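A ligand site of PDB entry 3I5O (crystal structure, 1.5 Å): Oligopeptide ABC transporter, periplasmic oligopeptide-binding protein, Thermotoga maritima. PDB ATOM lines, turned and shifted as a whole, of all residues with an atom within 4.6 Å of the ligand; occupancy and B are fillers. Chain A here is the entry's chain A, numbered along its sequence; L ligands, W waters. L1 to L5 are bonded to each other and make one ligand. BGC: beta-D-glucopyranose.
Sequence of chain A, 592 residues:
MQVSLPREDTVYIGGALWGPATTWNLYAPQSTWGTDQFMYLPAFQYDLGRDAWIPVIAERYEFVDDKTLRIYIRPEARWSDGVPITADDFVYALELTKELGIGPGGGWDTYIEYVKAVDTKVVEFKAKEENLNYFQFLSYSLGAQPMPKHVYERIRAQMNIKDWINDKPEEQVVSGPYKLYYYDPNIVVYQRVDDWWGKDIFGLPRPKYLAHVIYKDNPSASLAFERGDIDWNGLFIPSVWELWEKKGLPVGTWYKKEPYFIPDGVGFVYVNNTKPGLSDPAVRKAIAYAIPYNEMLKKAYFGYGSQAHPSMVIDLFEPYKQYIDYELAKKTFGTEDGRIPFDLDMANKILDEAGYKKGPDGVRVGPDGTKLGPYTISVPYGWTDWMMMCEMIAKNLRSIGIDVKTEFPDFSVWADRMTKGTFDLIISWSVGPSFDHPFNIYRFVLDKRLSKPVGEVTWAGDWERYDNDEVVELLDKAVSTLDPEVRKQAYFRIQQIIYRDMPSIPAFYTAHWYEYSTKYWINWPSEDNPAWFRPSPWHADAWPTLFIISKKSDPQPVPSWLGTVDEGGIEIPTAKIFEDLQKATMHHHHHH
An oxygen (O1) of BGC L1 sits at hydrogen-bond distance from the backbone carbonyl oxygen (O) of Gly 103 (2.6 Å).
OD1 of Asp 385 lies within hydrogen-bond range of O4 of BGC L5 (2.6 Å).
The side-chain amide oxygen of Asn 218 is in hydrogen-bond range of an oxygen (O3) of BGC L5, at 2.7 Å.
O2 of BGC L5 sits at hydrogen-bond distance from O of Gly 15 (2.8 Å).
An oxygen (O3) of BGC L5 is in hydrogen-bond range of the backbone NH (N) of Phe 236, 2.8 Å away.
The indole nitrogen (NE1) of Trp 513 sits at hydrogen-bond distance from an oxygen (O6) of BGC L5 (2.9 Å).
An oxygen (O6) of BGC L1 lies within hydrogen-bond range of the backbone NH of Gly 105 (2.9 Å).
An oxygen (O2) of BGC L1 lies within hydrogen-bond range of the backbone NH (N) of Ala 460.
The indole nitrogen (NE1) of Trp 18 lies within hydrogen-bond range of an oxygen (O2) of BGC L5.
The side-chain carboxylate of Asp 264 is in hydrogen-bond range of an oxygen (O6) of BGC L3 (2.9 Å).
The backbone carbonyl oxygen (O) of Trp 459 lies close to an oxygen (O2) of BGC L1, at 3.4 Å.
An oxygen (O1) of BGC L1 lies within hydrogen-bond range of the backbone NH of Gly 106 (2.9 Å).
An oxygen (O6) of BGC L4 is in hydrogen-bond range of the backbone carbonyl oxygen (O) of Ala 16.
NE1 of Trp 429 lies within hydrogen-bond range of O6 of BGC L2 (3.2 Å).
O of Gly 234 is in hydrogen-bond range of O2 of BGC L5 (3.2 Å).
An oxygen (O4) of BGC L4 lies within hydrogen-bond range of the indole nitrogen of Trp 538 (3.3 Å).
NE1 of Trp 386 is in hydrogen-bond range of O6 of BGC L5 (3.3 Å).
Water W13 lies within hydrogen-bond range of an oxygen (O4) of BGC L2 (2.6 Å), the backbone NH (N) of Ala 540 (2.9 Å) and the backbone carbonyl oxygen (O) of Trp 538 (3.0 Å).
Water W3 lies within hydrogen-bond range of NE2 of Gln 145 and O6 of BGC L1.
Water W16 lies within hydrogen-bond range of the backbone carbonyl oxygen (O) of Trp 459 and an oxygen (O6) of BGC L2.
Water W8 bridges an oxygen (O6) of BGC L4 and the backbone carbonyl oxygen of Ala 16.
Water W9 lies within hydrogen-bond range of an oxygen (O2) of BGC L1 (2.8 Å), the backbone NH of Trp 459 (2.8 Å) and the backbone NH of Ala 460 (3.4 Å).
Water W15 lies within hydrogen-bond range of O3 of BGC L2 (2.8 Å) and N of Ala 540 (3.0 Å).
ND2 of Asn 218 is in hydrogen-bond range of OG1 of Thr 384, 3.1 Å away.
The backbone carbonyl oxygen (O) of Gly 15 is in hydrogen-bond range of the indole nitrogen (NE1) of Trp 18, at 3.4 Å.
The indole nitrogen (NE1) of Trp 538 sits at hydrogen-bond distance from the backbone carbonyl oxygen (O) of Gly 234, at 3.0 Å.
CA of Pro 104 touches O5 of BGC L1 (3.4 Å).
CD1 of Leu 235 touches O3 of BGC L5, 3.4 Å away.
CA of Trp 383 touches O4 of BGC L5, 3.4 Å away.
N of Thr 384 touches O4 of BGC L5 (3.98 Å).
CD2 of His 539 touches O6 of BGC L3 (3.9 Å).
Ala 540 touches the ligand.
Hydrophobic or aromatic side chains within 4 Å of the ligand: Trp 18, Leu 235, Phe 236, Trp 383, Trp 386, Trp 429, Trp 459, Ala 460, Trp 513, Trp 538, His 539 and Ala 540.
23 residues have an atom within 4 Å of the ligand: Gly 15, Ala 16, Trp 18, Gly 103, Pro 104, Gly 105, Gly 106, Asn 218, Gly 234, Leu 235, Phe 236, Asp 264, Trp 383, Thr 384, Asp 385, Trp 386, Trp 429, Trp 459, Ala 460, Trp 513, Trp 538, His 539 and Ala 540.
Along chain A the residues within 4 Å of the ligand span positions 15 to 540.
The nearest printed residue that does not touch the ligand is Gln 145 (4.3 Å).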
ATOM      1  N   GLY A  15       6.813  27.890  10.262  1.00  0.00           N
ATOM      2  CA  GLY A  15       6.026  27.225  11.282  1.00  0.00           C
ATOM      3  C   GLY A  15       6.773  26.374  12.303  1.00  0.00           C
ATOM      4  O   GLY A  15       6.128  25.687  13.099  1.00  0.00           O
ATOM      5  N   ALA A  16       8.098  26.430  12.326  1.00  0.00           N
ATOM      6  CA  ALA A  16       8.854  25.570  13.262  1.00  0.00           C
ATOM      7  C   ALA A  16       9.561  26.369  14.350  1.00  0.00           C
ATOM      8  O   ALA A  16       9.743  25.902  15.482  1.00  0.00           O
ATOM      9  CB  ALA A  16       9.859  24.692  12.488  1.00  0.00           C
ATOM     10  N   TRP A  18       9.373  29.860  16.389  1.00  0.00           N
ATOM     11  CA  TRP A  18       8.542  30.977  16.832  1.00  0.00           C
ATOM     12  C   TRP A  18       9.256  31.697  17.960  1.00  0.00           C
ATOM     13  O   TRP A  18       9.820  31.064  18.844  1.00  0.00           O
ATOM     14  CB  TRP A  18       7.205  30.452  17.332  1.00  0.00           C
ATOM     15  CG  TRP A  18       6.356  29.858  16.260  1.00  0.00           C
ATOM     16  CD1 TRP A  18       6.219  28.537  15.974  1.00  0.00           C
ATOM     17  CD2 TRP A  18       5.520  30.569  15.351  1.00  0.00           C
ATOM     18  NE1 TRP A  18       5.349  28.381  14.933  1.00  0.00           N
ATOM     19  CE2 TRP A  18       4.902  29.612  14.530  1.00  0.00           C
ATOM     20  CE3 TRP A  18       5.225  31.926  15.147  1.00  0.00           C
ATOM     21  CZ2 TRP A  18       3.998  29.952  13.518  1.00  0.00           C
ATOM     22  CZ3 TRP A  18       4.318  32.264  14.144  1.00  0.00           C
ATOM     23  CH2 TRP A  18       3.719  31.284  13.347  1.00  0.00           C
ATOM     24  N   ASP A  36      18.135  20.074  18.104  1.00  0.00           N
ATOM     25  CA  ASP A  36      17.921  18.652  18.288  1.00  0.00           C
ATOM     26  C   ASP A  36      17.650  17.991  16.940  1.00  0.00           C
ATOM     27  O   ASP A  36      18.165  16.926  16.634  1.00  0.00           O
ATOM     28  CB  ASP A  36      16.754  18.418  19.245  1.00  0.00           C
ATOM     29  CG  ASP A  36      16.897  17.134  20.049  1.00  0.00           C
ATOM     30  OD1 ASP A  36      17.720  16.277  19.680  1.00  0.00           O
ATOM     31  OD2 ASP A  36      16.180  16.981  21.062  1.00  0.00           O
ATOM     32  N   GLY A 103      18.140  18.411  30.182  1.00  0.00           N
ATOM     33  CA  GLY A 103      18.939  17.936  29.075  1.00  0.00           C
ATOM     34  C   GLY A 103      18.316  16.714  28.456  1.00  0.00           C
ATOM     35  O   GLY A 103      17.323  16.199  28.949  1.00  0.00           O
ATOM     36  N   PRO A 104      18.919  16.221  27.362  1.00  0.00           N
ATOM     37  CA  PRO A 104      18.387  15.084  26.599  1.00  0.00           C
ATOM     38  C   PRO A 104      18.382  13.785  27.402  1.00  0.00           C
ATOM     39  O   PRO A 104      19.312  13.514  28.168  1.00  0.00           O
ATOM     40  CB  PRO A 104      19.353  14.974  25.423  1.00  0.00           C
ATOM     41  CG  PRO A 104      20.602  15.678  25.859  1.00  0.00           C
ATOM     42  CD  PRO A 104      20.155  16.766  26.777  1.00  0.00           C
ATOM     43  N   GLY A 105      17.328  12.995  27.221  1.00  0.00           N
ATOM     44  CA  GLY A 105      17.248  11.692  27.856  1.00  0.00           C
ATOM     45  C   GLY A 105      16.767  11.768  29.292  1.00  0.00           C
ATOM     46  O   GLY A 105      17.058  10.878  30.091  1.00  0.00           O
ATOM     47  N   GLY A 106      16.031  12.825  29.637  1.00  0.00           N
ATOM     48  CA  GLY A 106      15.530  12.997  30.990  1.00  0.00           C
ATOM     49  C   GLY A 106      14.730  11.799  31.471  1.00  0.00           C
ATOM     50  O   GLY A 106      13.893  11.268  30.750  1.00  0.00           O
ATOM     51  N   GLN A 145      21.252   9.725  22.594  1.00  0.00           N
ATOM     52  CA  GLN A 145      21.993  10.729  21.846  1.00  0.00           C
ATOM     53  C   GLN A 145      23.292  11.034  22.594  1.00  0.00           C
ATOM     54  O   GLN A 145      23.268  11.372  23.771  1.00  0.00           O
ATOM     55  CB  GLN A 145      21.178  12.012  21.693  1.00  0.00           C
ATOM     56  CG  GLN A 145      19.818  11.824  21.036  1.00  0.00           C
ATOM     57  CD  GLN A 145      19.084  13.145  20.832  1.00  0.00           C
ATOM     58  OE1 GLN A 145      19.483  13.966  20.023  1.00  0.00           O
ATOM     59  NE2 GLN A 145      18.003  13.331  21.574  1.00  0.00           N
ATOM     60  N   ASN A 218       0.740  33.483  12.079  1.00  0.00           N
ATOM     61  CA  ASN A 218       0.321  32.616  10.969  1.00  0.00           C
ATOM     62  C   ASN A 218       0.037  33.370   9.657  1.00  0.00           C
ATOM     63  O   ASN A 218       0.499  32.945   8.605  1.00  0.00           O
ATOM     64  CB  ASN A 218      -0.867  31.741  11.361  1.00  0.00           C
ATOM     65  CG  ASN A 218      -0.439  30.569  12.223  1.00  0.00           C
ATOM     66  OD1 ASN A 218       0.741  30.217  12.260  1.00  0.00           O
ATOM     67  ND2 ASN A 218      -1.398  29.963  12.914  1.00  0.00           N
ATOM     68  N   GLY A 234       5.359  24.000   8.363  1.00  0.00           N
ATOM     69  CA  GLY A 234       4.732  23.243   9.441  1.00  0.00           C
ATOM     70  C   GLY A 234       3.701  24.108  10.139  1.00  0.00           C
ATOM     71  O   GLY A 234       3.622  24.205  11.375  1.00  0.00           O
ATOM     72  N   LEU A 235       2.871  24.749   9.314  1.00  0.00           N
ATOM     73  CA  LEU A 235       1.963  25.799   9.759  1.00  0.00           C
ATOM     74  C   LEU A 235       0.511  25.353   9.782  1.00  0.00           C
ATOM     75  O   LEU A 235       0.067  24.529   8.976  1.00  0.00           O
ATOM     76  CB  LEU A 235       2.073  26.983   8.785  1.00  0.00           C
ATOM     77  CG  LEU A 235       1.826  28.405   9.282  1.00  0.00           C
ATOM     78  CD1 LEU A 235       2.952  28.895  10.171  1.00  0.00           C
ATOM     79  CD2 LEU A 235       1.652  29.344   8.081  1.00  0.00           C
ATOM     80  N   PHE A 236      -0.265  25.925  10.691  1.00  0.00           N
ATOM     81  CA  PHE A 236      -1.700  25.918  10.532  1.00  0.00           C
ATOM     82  C   PHE A 236      -2.062  26.882   9.411  1.00  0.00           C
ATOM     83  O   PHE A 236      -1.624  28.026   9.418  1.00  0.00           O
ATOM     84  CB  PHE A 236      -2.400  26.354  11.828  1.00  0.00           C
ATOM     85  CG  PHE A 236      -3.837  26.765  11.606  1.00  0.00           C
ATOM     86  CD1 PHE A 236      -4.824  25.801  11.476  1.00  0.00           C
ATOM     87  CD2 PHE A 236      -4.182  28.101  11.477  1.00  0.00           C
ATOM     88  CE1 PHE A 236      -6.174  26.171  11.244  1.00  0.00           C
ATOM     89  CE2 PHE A 236      -5.520  28.477  11.250  1.00  0.00           C
ATOM     90  CZ  PHE A 236      -6.510  27.511  11.130  1.00  0.00           C
ATOM     91  N   ASP A 264      -0.193  14.105  14.665  1.00  0.00           N
ATOM     92  CA  ASP A 264       1.081  14.213  15.373  1.00  0.00           C
ATOM     93  C   ASP A 264       1.041  13.596  16.763  1.00  0.00           C
ATOM     94  O   ASP A 264       1.979  12.896  17.159  1.00  0.00           O
ATOM     95  CB  ASP A 264       1.504  15.668  15.507  1.00  0.00           C
ATOM     96  CG  ASP A 264       2.957  15.783  15.933  1.00  0.00           C
ATOM     97  OD1 ASP A 264       3.843  15.380  15.152  1.00  0.00           O
ATOM     98  OD2 ASP A 264       3.230  16.250  17.068  1.00  0.00           O
ATOM     99  N   TYR A 301     -10.336  24.762  13.927  1.00  0.00           N
ATOM    100  CA  TYR A 301      -9.327  23.798  13.503  1.00  0.00           C
ATOM    101  C   TYR A 301      -9.616  23.232  12.103  1.00  0.00           C
ATOM    102  O   TYR A 301      -8.894  22.355  11.640  1.00  0.00           O
ATOM    103  CB  TYR A 301      -9.235  22.658  14.514  1.00  0.00           C
ATOM    104  CG  TYR A 301      -7.847  22.076  14.736  1.00  0.00           C
ATOM    105  CD1 TYR A 301      -7.627  20.694  14.627  1.00  0.00           C
ATOM    106  CD2 TYR A 301      -6.769  22.875  15.079  1.00  0.00           C
ATOM    107  CE1 TYR A 301      -6.361  20.135  14.845  1.00  0.00           C
ATOM    108  CE2 TYR A 301      -5.493  22.320  15.311  1.00  0.00           C
ATOM    109  CZ  TYR A 301      -5.310  20.951  15.192  1.00  0.00           C
ATOM    110  OH  TYR A 301      -4.064  20.389  15.401  1.00  0.00           O
ATOM    111  N   TRP A 383      -0.324  31.934  16.985  1.00  0.00           N
ATOM    112  CA  TRP A 383      -0.830  30.590  16.738  1.00  0.00           C
ATOM    113  C   TRP A 383      -2.359  30.651  16.647  1.00  0.00           C
ATOM    114  O   TRP A 383      -3.082  30.239  17.560  1.00  0.00           O
ATOM    115  CB  TRP A 383      -0.385  29.623  17.834  1.00  0.00           C
ATOM    116  CG  TRP A 383       1.086  29.300  17.806  1.00  0.00           C
ATOM    117  CD1 TRP A 383       2.085  30.046  17.223  1.00  0.00           C
ATOM    118  CD2 TRP A 383       1.731  28.180  18.421  1.00  0.00           C
ATOM    119  NE1 TRP A 383       3.304  29.430  17.422  1.00  0.00           N
ATOM    120  CE2 TRP A 383       3.110  28.279  18.147  1.00  0.00           C
ATOM    121  CE3 TRP A 383       1.269  27.077  19.148  1.00  0.00           C
ATOM    122  CZ2 TRP A 383       4.030  27.342  18.595  1.00  0.00           C
ATOM    123  CZ3 TRP A 383       2.188  26.140  19.595  1.00  0.00           C
ATOM    124  CH2 TRP A 383       3.550  26.279  19.314  1.00  0.00           C
ATOM    125  N   THR A 384      -2.834  31.192  15.526  1.00  0.00           N
ATOM    126  CA  THR A 384      -4.213  31.664  15.445  1.00  0.00           C
ATOM    127  C   THR A 384      -5.311  30.632  15.673  1.00  0.00           C
ATOM    128  O   THR A 384      -6.367  30.981  16.209  1.00  0.00           O
ATOM    129  CB  THR A 384      -4.448  32.372  14.098  1.00  0.00           C
ATOM    130  OG1 THR A 384      -4.029  31.506  13.044  1.00  0.00           O
ATOM    131  CG2 THR A 384      -3.634  33.657  14.029  1.00  0.00           C
ATOM    132  N   ASP A 385      -5.098  29.382  15.276  1.00  0.00           N
ATOM    133  CA  ASP A 385      -6.077  28.325  15.519  1.00  0.00           C
ATOM    134  C   ASP A 385      -6.227  28.048  17.018  1.00  0.00           C
ATOM    135  O   ASP A 385      -7.346  27.987  17.542  1.00  0.00           O
ATOM    136  CB  ASP A 385      -5.711  27.046  14.770  1.00  0.00           C
ATOM    137  CG  ASP A 385      -4.293  26.533  15.093  1.00  0.00           C
ATOM    138  OD1 ASP A 385      -3.378  27.360  15.309  1.00  0.00           O
ATOM    139  OD2 ASP A 385      -4.107  25.307  15.103  1.00  0.00           O
ATOM    140  N   TRP A 386      -5.107  27.881  17.699  1.00  0.00           N
ATOM    141  CA  TRP A 386      -5.143  27.667  19.143  1.00  0.00           C
ATOM    142  C   TRP A 386      -5.673  28.899  19.868  1.00  0.00           C
ATOM    143  O   TRP A 386      -6.367  28.782  20.886  1.00  0.00           O
ATOM    144  CB  TRP A 386      -3.751  27.313  19.675  1.00  0.00           C
ATOM    145  CG  TRP A 386      -3.355  25.885  19.424  1.00  0.00           C
ATOM    146  CD1 TRP A 386      -3.933  25.007  18.559  1.00  0.00           C
ATOM    147  CD2 TRP A 386      -2.291  25.174  20.067  1.00  0.00           C
ATOM    148  NE1 TRP A 386      -3.284  23.796  18.615  1.00  0.00           N
ATOM    149  CE2 TRP A 386      -2.278  23.868  19.535  1.00  0.00           C
ATOM    150  CE3 TRP A 386      -1.341  25.512  21.045  1.00  0.00           C
ATOM    151  CZ2 TRP A 386      -1.334  22.897  19.929  1.00  0.00           C
ATOM    152  CZ3 TRP A 386      -0.403  24.554  21.440  1.00  0.00           C
ATOM    153  CH2 TRP A 386      -0.427  23.260  20.897  1.00  0.00           C
ATOM    154  N   TRP A 429       1.093  20.468  23.452  1.00  0.00           N
ATOM    155  CA  TRP A 429       1.239  19.121  22.903  1.00  0.00           C
ATOM    156  C   TRP A 429       1.578  18.097  23.993  1.00  0.00           C
ATOM    157  O   TRP A 429       1.618  18.436  25.182  1.00  0.00           O
ATOM    158  CB  TRP A 429       2.324  19.105  21.811  1.00  0.00           C
ATOM    159  CG  TRP A 429       3.708  19.455  22.305  1.00  0.00           C
ATOM    160  CD1 TRP A 429       4.632  18.599  22.836  1.00  0.00           C
ATOM    161  CD2 TRP A 429       4.324  20.760  22.302  1.00  0.00           C
ATOM    162  NE1 TRP A 429       5.796  19.276  23.151  1.00  0.00           N
ATOM    163  CE2 TRP A 429       5.631  20.601  22.835  1.00  0.00           C
ATOM    164  CE3 TRP A 429       3.915  22.027  21.888  1.00  0.00           C
ATOM    165  CZ2 TRP A 429       6.508  21.674  22.981  1.00  0.00           C
ATOM    166  CZ3 TRP A 429       4.790  23.091  22.032  1.00  0.00           C
ATOM    167  CH2 TRP A 429       6.074  22.903  22.572  1.00  0.00           C
ATOM    168  N   TRP A 459      11.102  20.031  30.447  1.00  0.00           N
ATOM    169  CA  TRP A 459      10.609  19.668  29.127  1.00  0.00           C
ATOM    170  C   TRP A 459      10.300  18.176  29.090  1.00  0.00           C
ATOM    171  O   TRP A 459       9.745  17.682  28.109  1.00  0.00           O
ATOM    172  CB  TRP A 459      11.648  19.981  28.055  1.00  0.00           C
ATOM    173  CG  TRP A 459      11.818  21.429  27.753  1.00  0.00           C
ATOM    174  CD1 TRP A 459      12.813  22.253  28.190  1.00  0.00           C
ATOM    175  CD2 TRP A 459      10.983  22.229  26.906  1.00  0.00           C
ATOM    176  NE1 TRP A 459      12.636  23.520  27.685  1.00  0.00           N
ATOM    177  CE2 TRP A 459      11.524  23.533  26.898  1.00  0.00           C
ATOM    178  CE3 TRP A 459       9.818  21.970  26.172  1.00  0.00           C
ATOM    179  CZ2 TRP A 459      10.951  24.575  26.162  1.00  0.00           C
ATOM    180  CZ3 TRP A 459       9.244  23.012  25.436  1.00  0.00           C
ATOM    181  CH2 TRP A 459       9.807  24.296  25.442  1.00  0.00           C
ATOM    182  N   ALA A 460      10.653  17.465  30.165  1.00  0.00           N
ATOM    183  CA  ALA A 460      10.561  16.009  30.180  1.00  0.00           C
ATOM    184  C   ALA A 460       9.141  15.479  30.380  1.00  0.00           C
ATOM    185  O   ALA A 460       8.834  14.359  29.969  1.00  0.00           O
ATOM    186  CB  ALA A 460      11.510  15.419  31.230  1.00  0.00           C
ATOM    187  N   TRP A 513       1.342  19.259  11.177  1.00  0.00           N
ATOM    188  CA  TRP A 513       1.367  20.317  10.157  1.00  0.00           C
ATOM    189  C   TRP A 513       2.511  20.089   9.180  1.00  0.00           C
ATOM    190  O   TRP A 513       3.675  19.977   9.575  1.00  0.00           O
ATOM    191  CB  TRP A 513       1.565  21.712  10.750  1.00  0.00           C
ATOM    192  CG  TRP A 513       0.536  22.145  11.768  1.00  0.00           C
ATOM    193  CD1 TRP A 513       0.795  22.633  13.021  1.00  0.00           C
ATOM    194  CD2 TRP A 513      -0.884  22.129  11.623  1.00  0.00           C
ATOM    195  NE1 TRP A 513      -0.381  22.907  13.662  1.00  0.00           N
ATOM    196  CE2 TRP A 513      -1.433  22.616  12.831  1.00  0.00           C
ATOM    197  CE3 TRP A 513      -1.755  21.756  10.590  1.00  0.00           C
ATOM    198  CZ2 TRP A 513      -2.809  22.729  13.043  1.00  0.00           C
ATOM    199  CZ3 TRP A 513      -3.131  21.868  10.801  1.00  0.00           C
ATOM    200  CH2 TRP A 513      -3.638  22.354  12.013  1.00  0.00           C
ATOM    201  N   TRP A 538       9.236  20.811  12.179  1.00  0.00           N
ATOM    202  CA  TRP A 538       9.493  20.932  13.613  1.00  0.00           C
ATOM    203  C   TRP A 538       9.587  19.600  14.335  1.00  0.00           C
ATOM    204  O   TRP A 538       9.940  19.570  15.512  1.00  0.00           O
ATOM    205  CB  TRP A 538       8.452  21.825  14.302  1.00  0.00           C
ATOM    206  CG  TRP A 538       7.022  21.674  13.866  1.00  0.00           C
ATOM    207  CD1 TRP A 538       6.303  22.566  13.112  1.00  0.00           C
ATOM    208  CD2 TRP A 538       6.113  20.598  14.183  1.00  0.00           C
ATOM    209  NE1 TRP A 538       5.022  22.111  12.944  1.00  0.00           N
ATOM    210  CE2 TRP A 538       4.870  20.913  13.577  1.00  0.00           C
ATOM    211  CE3 TRP A 538       6.223  19.410  14.910  1.00  0.00           C
ATOM    212  CZ2 TRP A 538       3.742  20.077  13.684  1.00  0.00           C
ATOM    213  CZ3 TRP A 538       5.107  18.573  15.010  1.00  0.00           C
ATOM    214  CH2 TRP A 538       3.874  18.918  14.403  1.00  0.00           C
ATOM    215  N   HIS A 539       9.299  18.496  13.643  1.00  0.00           N
ATOM    216  CA  HIS A 539       9.272  17.219  14.356  1.00  0.00           C
ATOM    217  C   HIS A 539      10.667  16.741  14.765  1.00  0.00           C
ATOM    218  O   HIS A 539      11.644  16.923  14.033  1.00  0.00           O
ATOM    219  CB  HIS A 539       8.557  16.145  13.542  1.00  0.00           C
ATOM    220  CG  HIS A 539       8.094  14.992  14.366  1.00  0.00           C
ATOM    221  ND1 HIS A 539       8.912  13.916  14.651  1.00  0.00           N
ATOM    222  CD2 HIS A 539       6.923  14.771  15.000  1.00  0.00           C
ATOM    223  CE1 HIS A 539       8.253  13.068  15.418  1.00  0.00           C
ATOM    224  NE2 HIS A 539       7.037  13.564  15.648  1.00  0.00           N
ATOM    225  N   ALA A 540      10.759  16.152  15.948  1.00  0.00           N
ATOM    226  CA  ALA A 540      12.021  15.608  16.437  1.00  0.00           C
ATOM    227  C   ALA A 540      12.698  14.695  15.421  1.00  0.00           C
ATOM    228  O   ALA A 540      13.917  14.599  15.363  1.00  0.00           O
ATOM    229  CB  ALA A 540      11.778  14.828  17.720  1.00  0.00           C
HETATM  230  C2  BGC L   1      13.853  16.801  27.579  1.00  0.00           C
HETATM  231  C3  BGC L   1      13.014  16.756  26.324  1.00  0.00           C
HETATM  232  C4  BGC L   1      13.544  15.764  25.305  1.00  0.00           C
HETATM  233  C5  BGC L   1      14.274  14.538  25.840  1.00  0.00           C
HETATM  234  C6  BGC L   1      15.265  14.020  24.813  1.00  0.00           C
HETATM  235  C1  BGC L   1      14.153  15.393  28.055  1.00  0.00           C
HETATM  236  O1  BGC L   1      14.883  15.509  29.276  1.00  0.00           O
HETATM  237  O2  BGC L   1      13.124  17.501  28.597  1.00  0.00           O
HETATM  238  O3  BGC L   1      13.004  18.074  25.758  1.00  0.00           O
HETATM  239  O4  BGC L   1      12.415  15.268  24.577  1.00  0.00           O
HETATM  240  O5  BGC L   1      14.980  14.826  27.046  1.00  0.00           O
HETATM  241  O6  BGC L   1      15.461  12.625  25.050  1.00  0.00           O
HETATM  242  C2  BGC L   2      11.253  15.579  22.290  1.00  0.00           C
HETATM  243  C3  BGC L   2      10.712  16.319  21.101  1.00  0.00           C
HETATM  244  C4  BGC L   2      10.144  17.633  21.592  1.00  0.00           C
HETATM  245  C5  BGC L   2      10.917  18.418  22.667  1.00  0.00           C
HETATM  246  C6  BGC L   2      10.144  19.570  23.301  1.00  0.00           C
HETATM  247  C1  BGC L   2      12.157  16.631  22.906  1.00  0.00           C
HETATM  248  O2  BGC L   2      11.997  14.439  21.854  1.00  0.00           O
HETATM  249  O3  BGC L   2       9.717  15.549  20.415  1.00  0.00           O
HETATM  250  O4  BGC L   2      10.281  18.409  20.411  1.00  0.00           O
HETATM  251  O5  BGC L   2      11.355  17.514  23.667  1.00  0.00           O
HETATM  252  O6  BGC L   2       8.897  19.101  23.823  1.00  0.00           O
HETATM  253  C2  BGC L   3       8.905  20.342  19.420  1.00  0.00           C
HETATM  254  C3  BGC L   3       7.609  21.025  19.068  1.00  0.00           C
HETATM  255  C4  BGC L   3       6.568  19.965  18.737  1.00  0.00           C
HETATM  256  C5  BGC L   3       6.461  18.784  19.702  1.00  0.00           C
HETATM  257  C6  BGC L   3       5.484  17.704  19.238  1.00  0.00           C
HETATM  258  C1  BGC L   3       8.426  19.392  20.477  1.00  0.00           C
HETATM  259  O2  BGC L   3       9.826  21.260  20.004  1.00  0.00           O
HETATM  260  O3  BGC L   3       7.886  21.892  17.966  1.00  0.00           O
HETATM  261  O4  BGC L   3       5.312  20.568  18.933  1.00  0.00           O
HETATM  262  O5  BGC L   3       7.773  18.291  19.841  1.00  0.00           O
HETATM  263  O6  BGC L   3       5.876  17.134  17.978  1.00  0.00           O
HETATM  264  C2  BGC L   4       3.267  21.470  17.727  1.00  0.00           C
HETATM  265  C3  BGC L   4       2.723  22.209  16.547  1.00  0.00           C
HETATM  266  C4  BGC L   4       3.540  23.473  16.400  1.00  0.00           C
HETATM  267  C5  BGC L   4       5.052  23.363  16.453  1.00  0.00           C
HETATM  268  C6  BGC L   4       5.724  24.728  16.558  1.00  0.00           C
HETATM  269  C1  BGC L   4       4.711  21.359  17.312  1.00  0.00           C
HETATM  270  O2  BGC L   4       2.650  20.187  17.799  1.00  0.00           O
HETATM  271  O3  BGC L   4       1.348  22.489  16.806  1.00  0.00           O
HETATM  272  O4  BGC L   4       3.202  23.900  15.075  1.00  0.00           O
HETATM  273  O5  BGC L   4       5.360  22.586  17.606  1.00  0.00           O
HETATM  274  O6  BGC L   4       7.147  24.591  16.422  1.00  0.00           O
HETATM  275  C2  BGC L   5       2.269  26.051  13.941  1.00  0.00           C
HETATM  276  C3  BGC L   5       1.247  27.147  13.946  1.00  0.00           C
HETATM  277  C4  BGC L   5      -0.058  26.669  14.586  1.00  0.00           C
HETATM  278  C5  BGC L   5       0.189  25.999  15.935  1.00  0.00           C
HETATM  279  C6  BGC L   5      -1.070  25.393  16.565  1.00  0.00           C
HETATM  280  C1  BGC L   5       2.379  25.739  15.405  1.00  0.00           C
HETATM  281  O2  BGC L   5       3.548  26.526  13.550  1.00  0.00           O
HETATM  282  O3  BGC L   5       1.010  27.558  12.588  1.00  0.00           O
HETATM  283  O4  BGC L   5      -0.879  27.796  14.808  1.00  0.00           O
HETATM  284  O5  BGC L   5       1.176  25.018  15.727  1.00  0.00           O
HETATM  285  O6  BGC L   5      -1.670  24.373  15.759  1.00  0.00           O
HETATM  286  O   HOH W   1      13.413  11.298  25.930  1.00  0.00           O
HETATM  287  O   HOH W   2      14.445  14.526  20.353  1.00  0.00           O
HETATM  288  O   HOH W   3      17.699  12.080  23.752  1.00  0.00           O
HETATM  289  O   HOH W   4      10.743  12.646  20.114  1.00  0.00           O
HETATM  290  O   HOH W   5      -2.232  21.865  16.552  1.00  0.00           O
HETATM  291  O   HOH W   6       7.771  14.691  22.144  1.00  0.00           O
HETATM  292  O   HOH W   7      -0.002  20.270  15.947  1.00  0.00           O
HETATM  293  O   HOH W   8       8.672  26.212  18.037  1.00  0.00           O
HETATM  294  O   HOH W   9      13.652  19.011  30.865  1.00  0.00           O
HETATM  295  O   HOH W  10      10.081  14.357  25.823  1.00  0.00           O
HETATM  296  O   HOH W  11      12.368  20.699  19.803  1.00  0.00           O
HETATM  297  O   HOH W  12      11.966  12.118  23.489  1.00  0.00           O
HETATM  298  O   HOH W  13      11.050  18.224  17.917  1.00  0.00           O
HETATM  299  O   HOH W  14       9.295  24.170  20.069  1.00  0.00           O
HETATM  300  O   HOH W  15       8.505  15.991  17.879  1.00  0.00           O
HETATM  301  O   HOH W  16       9.037  17.164  25.676  1.00  0.00           O
